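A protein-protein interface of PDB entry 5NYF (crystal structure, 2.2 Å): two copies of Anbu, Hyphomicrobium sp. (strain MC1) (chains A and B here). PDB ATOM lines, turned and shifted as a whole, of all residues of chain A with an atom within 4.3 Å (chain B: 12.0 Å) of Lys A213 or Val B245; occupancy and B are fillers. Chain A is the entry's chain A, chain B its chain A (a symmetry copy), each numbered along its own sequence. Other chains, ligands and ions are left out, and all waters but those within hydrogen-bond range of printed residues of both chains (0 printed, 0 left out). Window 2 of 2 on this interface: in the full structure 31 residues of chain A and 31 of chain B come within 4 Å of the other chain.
O of Ile A197 lies within hydrogen-bond range of N of Ile A215, at 2.8 Å. N of Leu A199 is in hydrogen-bond range of O of Lys A213.
Val B245 touches Lys A213 (CG2 to NZ, 3.7 Å). Val B245 touches Ile A215. Tyr A221 touches Asp B244. C of Val B245 touches CB of Tyr A221, at 3.8 Å. Phe A222 touches Val B245. Leu A225 touches Ile B240 (CD1 to O, 3.5 Å). Leu A225 touches Phe B243 (CD1 to CB, 3.8 Å). Leu A225 touches Val B245 (CD2 to O, 3.8 Å).
Lys A213 touches one residue of chain B. Of the printed residues of chain A, Val B245 touches Lys A213, Ile A215, Tyr A221, Phe A222 and Leu A225. No residue of chain B comes within 4 Å of Asp A198. No residue of chain B comes within 4 Å of Leu A199. No residue of chain B comes within 4 Å of Glu A212. Arg A214 touches none of the printed residues of chain B. Ile A215 touches one residue of chain B. Of chain B, only Asp B244 and Val B245 come within 4 Å of Tyr A221. Printed residues of chain B within 4 Å of Leu A225: Ile B240, Phe B243 and Val B245. Of the printed residues of chain A, Phe B243 touches Leu A225. Printed residues of chain A within 4 Å of Asp B244: Tyr A221. Printed residues of chain A within 4 Å of Ile B240: Leu A225. Phe B237 touches none of the printed residues of chain A. Lys B239 touches none of the printed residues of chain A. The nearest residue of chain B that does not touch Lys A213 is Asp B244 (6.2 Å). The nearest residue of chain A that does not touch Val B245 is Leu A180 (4.04 Å). The nearest printed residue of chain A that does not touch Asp B244 is Phe A222 (4.9 Å).
Of the 9 printed residues of chain B, 4 touch a printed residue of chain A. Hydrophobic or aromatic side chains of chain B within 4 Å of the printed part of chain A: Ile B240, Phe B243 and Val B245. Of the 11 printed residues of chain A, 5 touch a printed residue of chain B. Hydrophobic or aromatic side chains of chain A within 4 Å of the printed part of chain B: Ile A215, Tyr A221 and Leu A225. Along chain A the printed residues that touch a printed residue of chain B span positions 213 to 225. Among the printed residues, 8 pairs touch across the chains. Among the printed residues, no Asp or Glu carboxylate lies within 4 Å of a Lys or Arg side-chain nitrogen of the other chain.
No position is printed for both chains. Of the 8 pairs that touch across the chains among the printed residues, none has its exchanged pair printed and touching as well.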
ATOM      1  N   LEU A 180      22.067 -28.307 -29.148  1.00  0.00           N
ATOM      2  CA  LEU A 180      22.348 -29.344 -28.142  1.00  0.00           C
ATOM      3  C   LEU A 180      21.260 -30.410 -28.030  1.00  0.00           C
ATOM      4  O   LEU A 180      21.574 -31.581 -27.813  1.00  0.00           O
ATOM      5  CB  LEU A 180      22.607 -28.726 -26.759  1.00  0.00           C
ATOM      6  CG  LEU A 180      23.974 -28.067 -26.562  1.00  0.00           C
ATOM      7  CD1 LEU A 180      24.001 -27.292 -25.253  1.00  0.00           C
ATOM      8  CD2 LEU A 180      25.100 -29.094 -26.600  1.00  0.00           C
ATOM      9  N   ILE A 197      30.389 -33.593 -26.395  1.00  0.00           N
ATOM     10  CA  ILE A 197      29.948 -32.422 -27.181  1.00  0.00           C
ATOM     11  C   ILE A 197      30.807 -31.184 -26.903  1.00  0.00           C
ATOM     12  O   ILE A 197      30.747 -30.613 -25.816  1.00  0.00           O
ATOM     13  CB  ILE A 197      28.449 -32.079 -26.963  1.00  0.00           C
ATOM     14  CG1 ILE A 197      27.559 -33.278 -27.329  1.00  0.00           C
ATOM     15  CG2 ILE A 197      28.044 -30.879 -27.820  1.00  0.00           C
ATOM     16  CD1 ILE A 197      26.128 -33.170 -26.844  1.00  0.00           C
ATOM     17  N   ASP A 198      31.588 -30.779 -27.906  1.00  0.00           N
ATOM     18  CA  ASP A 198      32.354 -29.533 -27.867  1.00  0.00           C
ATOM     19  C   ASP A 198      31.495 -28.424 -28.472  1.00  0.00           C
ATOM     20  O   ASP A 198      31.032 -28.550 -29.603  1.00  0.00           O
ATOM     21  CB  ASP A 198      33.670 -29.685 -28.650  1.00  0.00           C
ATOM     22  CG  ASP A 198      34.677 -28.563 -28.358  1.00  0.00           C
ATOM     23  OD1 ASP A 198      34.380 -27.647 -27.558  1.00  0.00           O
ATOM     24  OD2 ASP A 198      35.788 -28.605 -28.935  1.00  0.00           O
ATOM     25  N   LEU A 199      31.301 -27.345 -27.714  1.00  0.00           N
ATOM     26  CA  LEU A 199      30.400 -26.252 -28.073  1.00  0.00           C
ATOM     27  C   LEU A 199      31.167 -24.934 -28.088  1.00  0.00           C
ATOM     28  O   LEU A 199      31.812 -24.579 -27.099  1.00  0.00           O
ATOM     29  CB  LEU A 199      29.254 -26.169 -27.057  1.00  0.00           C
ATOM     30  CG  LEU A 199      28.296 -24.967 -27.099  1.00  0.00           C
ATOM     31  CD1 LEU A 199      27.488 -24.928 -28.389  1.00  0.00           C
ATOM     32  CD2 LEU A 199      27.371 -25.007 -25.892  1.00  0.00           C
ATOM     33  N   GLU A 212      33.685 -21.119 -24.880  1.00  0.00           N
ATOM     34  CA  GLU A 212      34.012 -22.472 -25.321  1.00  0.00           C
ATOM     35  C   GLU A 212      33.563 -23.410 -24.204  1.00  0.00           C
ATOM     36  O   GLU A 212      33.744 -23.087 -23.028  1.00  0.00           O
ATOM     37  CB  GLU A 212      35.525 -22.570 -25.557  1.00  0.00           C
ATOM     38  CG  GLU A 212      35.978 -23.707 -26.471  1.00  0.00           C
ATOM     39  CD  GLU A 212      36.258 -25.025 -25.764  1.00  0.00           C
ATOM     40  OE1 GLU A 212      36.253 -25.087 -24.513  1.00  0.00           O
ATOM     41  OE2 GLU A 212      36.501 -26.017 -26.484  1.00  0.00           O
ATOM     42  N   LYS A 213      32.970 -24.553 -24.551  1.00  0.00           N
ATOM     43  CA  LYS A 213      32.411 -25.452 -23.529  1.00  0.00           C
ATOM     44  C   LYS A 213      32.314 -26.919 -23.960  1.00  0.00           C
ATOM     45  O   LYS A 213      31.864 -27.220 -25.064  1.00  0.00           O
ATOM     46  CB  LYS A 213      31.028 -24.948 -23.097  1.00  0.00           C
ATOM     47  CG  LYS A 213      30.717 -25.190 -21.629  1.00  0.00           C
ATOM     48  CD  LYS A 213      29.524 -24.372 -21.156  1.00  0.00           C
ATOM     49  CE  LYS A 213      29.498 -24.280 -19.638  1.00  0.00           C
ATOM     50  NZ  LYS A 213      28.367 -23.452 -19.140  1.00  0.00           N
ATOM     51  N   ARG A 214      32.738 -27.816 -23.067  1.00  0.00           N
ATOM     52  CA  ARG A 214      32.603 -29.260 -23.248  1.00  0.00           C
ATOM     53  C   ARG A 214      31.414 -29.733 -22.414  1.00  0.00           C
ATOM     54  O   ARG A 214      31.431 -29.615 -21.192  1.00  0.00           O
ATOM     55  CB  ARG A 214      33.886 -29.973 -22.810  1.00  0.00           C
ATOM     56  CG  ARG A 214      33.865 -31.487 -22.986  1.00  0.00           C
ATOM     57  CD  ARG A 214      35.235 -32.105 -22.755  1.00  0.00           C
ATOM     58  NE  ARG A 214      36.158 -31.858 -23.866  1.00  0.00           N
ATOM     59  CZ  ARG A 214      36.134 -32.477 -25.051  1.00  0.00           C
ATOM     60  NH1 ARG A 214      37.039 -32.158 -25.974  1.00  0.00           N
ATOM     61  NH2 ARG A 214      35.219 -33.406 -25.335  1.00  0.00           N
ATOM     62  N   ILE A 215      30.385 -30.257 -23.079  1.00  0.00           N
ATOM     63  CA  ILE A 215      29.168 -30.726 -22.416  1.00  0.00           C
ATOM     64  C   ILE A 215      29.192 -32.247 -22.372  1.00  0.00           C
ATOM     65  O   ILE A 215      29.237 -32.902 -23.417  1.00  0.00           O
ATOM     66  CB  ILE A 215      27.882 -30.256 -23.144  1.00  0.00           C
ATOM     67  CG1 ILE A 215      27.919 -28.745 -23.436  1.00  0.00           C
ATOM     68  CG2 ILE A 215      26.639 -30.609 -22.331  1.00  0.00           C
ATOM     69  CD1 ILE A 215      28.097 -27.854 -22.219  1.00  0.00           C
ATOM     70  N   TYR A 221      22.707 -29.925 -15.986  1.00  0.00           N
ATOM     71  CA  TYR A 221      22.015 -28.844 -16.700  1.00  0.00           C
ATOM     72  C   TYR A 221      21.442 -29.376 -18.022  1.00  0.00           C
ATOM     73  O   TYR A 221      20.269 -29.169 -18.333  1.00  0.00           O
ATOM     74  CB  TYR A 221      22.964 -27.671 -16.994  1.00  0.00           C
ATOM     75  CG  TYR A 221      23.299 -26.770 -15.815  1.00  0.00           C
ATOM     76  CD1 TYR A 221      22.751 -25.487 -15.714  1.00  0.00           C
ATOM     77  CD2 TYR A 221      24.188 -27.181 -14.817  1.00  0.00           C
ATOM     78  CE1 TYR A 221      23.064 -24.651 -14.649  1.00  0.00           C
ATOM     79  CE2 TYR A 221      24.505 -26.351 -13.749  1.00  0.00           C
ATOM     80  CZ  TYR A 221      23.943 -25.088 -13.668  1.00  0.00           C
ATOM     81  OH  TYR A 221      24.258 -24.266 -12.611  1.00  0.00           O
ATOM     82  N   PHE A 222      22.287 -30.076 -18.778  1.00  0.00           N
ATOM     83  CA  PHE A 222      21.911 -30.659 -20.066  1.00  0.00           C
ATOM     84  C   PHE A 222      20.817 -31.723 -19.933  1.00  0.00           C
ATOM     85  O   PHE A 222      19.963 -31.843 -20.814  1.00  0.00           O
ATOM     86  CB  PHE A 222      23.157 -31.232 -20.761  1.00  0.00           C
ATOM     87  CG  PHE A 222      22.896 -31.834 -22.120  1.00  0.00           C
ATOM     88  CD1 PHE A 222      22.145 -31.156 -23.077  1.00  0.00           C
ATOM     89  CD2 PHE A 222      23.428 -33.078 -22.454  1.00  0.00           C
ATOM     90  CE1 PHE A 222      21.916 -31.715 -24.328  1.00  0.00           C
ATOM     91  CE2 PHE A 222      23.203 -33.640 -23.705  1.00  0.00           C
ATOM     92  CZ  PHE A 222      22.447 -32.957 -24.643  1.00  0.00           C
ATOM     93  N   LEU A 225      17.428 -29.821 -19.226  1.00  0.00           N
ATOM     94  CA  LEU A 225      16.950 -29.285 -20.508  1.00  0.00           C
ATOM     95  C   LEU A 225      16.331 -30.387 -21.373  1.00  0.00           C
ATOM     96  O   LEU A 225      15.251 -30.197 -21.942  1.00  0.00           O
ATOM     97  CB  LEU A 225      18.091 -28.600 -21.274  1.00  0.00           C
ATOM     98  CG  LEU A 225      17.758 -27.899 -22.597  1.00  0.00           C
ATOM     99  CD1 LEU A 225      16.888 -26.676 -22.357  1.00  0.00           C
ATOM    100  CD2 LEU A 225      19.033 -27.503 -23.332  1.00  0.00           C
ATOM    101  N   ARG B 164      10.659 -40.037 -27.408  1.00  0.00           N
ATOM    102  CA  ARG B 164      10.199 -39.173 -26.317  1.00  0.00           C
ATOM    103  C   ARG B 164       8.672 -39.149 -26.156  1.00  0.00           C
ATOM    104  O   ARG B 164       8.175 -39.036 -25.030  1.00  0.00           O
ATOM    105  CB  ARG B 164      10.729 -37.747 -26.521  1.00  0.00           C
ATOM    106  CG  ARG B 164      12.250 -37.633 -26.427  1.00  0.00           C
ATOM    107  CD  ARG B 164      12.730 -36.274 -26.920  1.00  0.00           C
ATOM    108  NE  ARG B 164      14.190 -36.133 -26.924  1.00  0.00           N
ATOM    109  CZ  ARG B 164      14.943 -35.658 -25.922  1.00  0.00           C
ATOM    110  NH1 ARG B 164      14.416 -35.259 -24.762  1.00  0.00           N
ATOM    111  NH2 ARG B 164      16.261 -35.584 -26.085  1.00  0.00           N
ATOM    112  N   PHE B 237       9.580 -25.162 -27.593  1.00  0.00           N
ATOM    113  CA  PHE B 237      10.943 -24.663 -27.428  1.00  0.00           C
ATOM    114  C   PHE B 237      10.978 -23.342 -26.658  1.00  0.00           C
ATOM    115  O   PHE B 237      11.832 -23.164 -25.798  1.00  0.00           O
ATOM    116  CB  PHE B 237      11.666 -24.506 -28.764  1.00  0.00           C
ATOM    117  CG  PHE B 237      13.107 -24.126 -28.607  1.00  0.00           C
ATOM    118  CD1 PHE B 237      14.022 -25.052 -28.131  1.00  0.00           C
ATOM    119  CD2 PHE B 237      13.541 -22.833 -28.876  1.00  0.00           C
ATOM    120  CE1 PHE B 237      15.346 -24.711 -27.958  1.00  0.00           C
ATOM    121  CE2 PHE B 237      14.865 -22.484 -28.704  1.00  0.00           C
ATOM    122  CZ  PHE B 237      15.770 -23.425 -28.246  1.00  0.00           C
ATOM    123  N   LYS B 239       9.051 -22.410 -24.310  1.00  0.00           N
ATOM    124  CA  LYS B 239       8.876 -22.748 -22.892  1.00  0.00           C
ATOM    125  C   LYS B 239      10.188 -23.199 -22.261  1.00  0.00           C
ATOM    126  O   LYS B 239      10.617 -22.640 -21.252  1.00  0.00           O
ATOM    127  CB  LYS B 239       7.814 -23.840 -22.716  1.00  0.00           C
ATOM    128  CG  LYS B 239       6.399 -23.396 -23.052  1.00  0.00           C
ATOM    129  CD  LYS B 239       5.732 -22.688 -21.880  1.00  0.00           C
ATOM    130  CE  LYS B 239       4.301 -22.282 -22.207  1.00  0.00           C
ATOM    131  NZ  LYS B 239       3.473 -22.143 -20.976  1.00  0.00           N
ATOM    132  N   ILE B 240      10.825 -24.196 -22.872  1.00  0.00           N
ATOM    133  CA  ILE B 240      12.051 -24.797 -22.321  1.00  0.00           C
ATOM    134  C   ILE B 240      13.310 -23.932 -22.436  1.00  0.00           C
ATOM    135  O   ILE B 240      14.331 -24.281 -21.849  1.00  0.00           O
ATOM    136  CB  ILE B 240      12.321 -26.225 -22.869  1.00  0.00           C
ATOM    137  CG1 ILE B 240      12.641 -26.229 -24.370  1.00  0.00           C
ATOM    138  CG2 ILE B 240      11.139 -27.135 -22.561  1.00  0.00           C
ATOM    139  CD1 ILE B 240      14.109 -26.124 -24.720  1.00  0.00           C
ATOM    140  N   GLU B 241      13.247 -22.835 -23.198  1.00  0.00           N
ATOM    141  CA  GLU B 241      14.307 -21.802 -23.219  1.00  0.00           C
ATOM    142  C   GLU B 241      14.675 -21.255 -21.837  1.00  0.00           C
ATOM    143  O   GLU B 241      15.788 -20.778 -21.648  1.00  0.00           O
ATOM    144  CB  GLU B 241      13.894 -20.616 -24.094  1.00  0.00           C
ATOM    145  CG  GLU B 241      14.184 -20.786 -25.573  1.00  0.00           C
ATOM    146  CD  GLU B 241      13.508 -19.733 -26.434  1.00  0.00           C
ATOM    147  OE1 GLU B 241      12.802 -18.851 -25.903  1.00  0.00           O
ATOM    148  OE2 GLU B 241      13.674 -19.792 -27.664  1.00  0.00           O
ATOM    149  N   GLU B 242      13.713 -21.286 -20.910  1.00  0.00           N
ATOM    150  CA  GLU B 242      13.930 -21.017 -19.476  1.00  0.00           C
ATOM    151  C   GLU B 242      15.170 -21.689 -18.903  1.00  0.00           C
ATOM    152  O   GLU B 242      15.881 -21.084 -18.115  1.00  0.00           O
ATOM    153  CB  GLU B 242      12.732 -21.520 -18.656  1.00  0.00           C
ATOM    154  CG  GLU B 242      11.471 -20.673 -18.749  1.00  0.00           C
ATOM    155  CD  GLU B 242      10.275 -21.298 -18.036  1.00  0.00           C
ATOM    156  OE1 GLU B 242      10.358 -22.471 -17.600  1.00  0.00           O
ATOM    157  OE2 GLU B 242       9.239 -20.606 -17.915  1.00  0.00           O
ATOM    158  N   PHE B 243      15.404 -22.946 -19.281  1.00  0.00           N
ATOM    159  CA  PHE B 243      16.477 -23.749 -18.692  1.00  0.00           C
ATOM    160  C   PHE B 243      17.844 -23.391 -19.272  1.00  0.00           C
ATOM    161  O   PHE B 243      17.956 -23.077 -20.455  1.00  0.00           O
ATOM    162  CB  PHE B 243      16.186 -25.243 -18.857  1.00  0.00           C
ATOM    163  CG  PHE B 243      14.995 -25.711 -18.065  1.00  0.00           C
ATOM    164  CD1 PHE B 243      15.151 -26.190 -16.765  1.00  0.00           C
ATOM    165  CD2 PHE B 243      13.712 -25.663 -18.609  1.00  0.00           C
ATOM    166  CE1 PHE B 243      14.054 -26.616 -16.027  1.00  0.00           C
ATOM    167  CE2 PHE B 243      12.612 -26.086 -17.876  1.00  0.00           C
ATOM    168  CZ  PHE B 243      12.782 -26.562 -16.583  1.00  0.00           C
ATOM    169  N   ASP B 244      18.874 -23.438 -18.426  1.00  0.00           N
ATOM    170  CA  ASP B 244      20.228 -23.037 -18.806  1.00  0.00           C
ATOM    171  C   ASP B 244      21.070 -24.236 -19.248  1.00  0.00           C
ATOM    172  O   ASP B 244      20.851 -25.356 -18.781  1.00  0.00           O
ATOM    173  CB  ASP B 244      20.914 -22.319 -17.638  1.00  0.00           C
ATOM    174  CG  ASP B 244      22.128 -21.494 -18.070  1.00  0.00           C
ATOM    175  OD1 ASP B 244      22.300 -21.215 -19.278  1.00  0.00           O
ATOM    176  OD2 ASP B 244      22.914 -21.111 -17.182  1.00  0.00           O
ATOM    177  N   VAL B 245      22.014 -23.963 -20.157  1.00  0.00           N
ATOM    178  CA  VAL B 245      22.993 -24.928 -20.711  1.00  0.00           C
ATOM    179  C   VAL B 245      22.598 -26.401 -20.565  1.00  0.00           C
ATOM    180  O   VAL B 245      22.376 -27.088 -21.560  1.00  0.00           O
ATOM    181  CB  VAL B 245      24.417 -24.681 -20.137  1.00  0.00           C
ATOM    182  CG1 VAL B 245      25.409 -25.745 -20.605  1.00  0.00           C
ATOM    183  CG2 VAL B 245      24.914 -23.297 -20.539  1.00  0.00           C
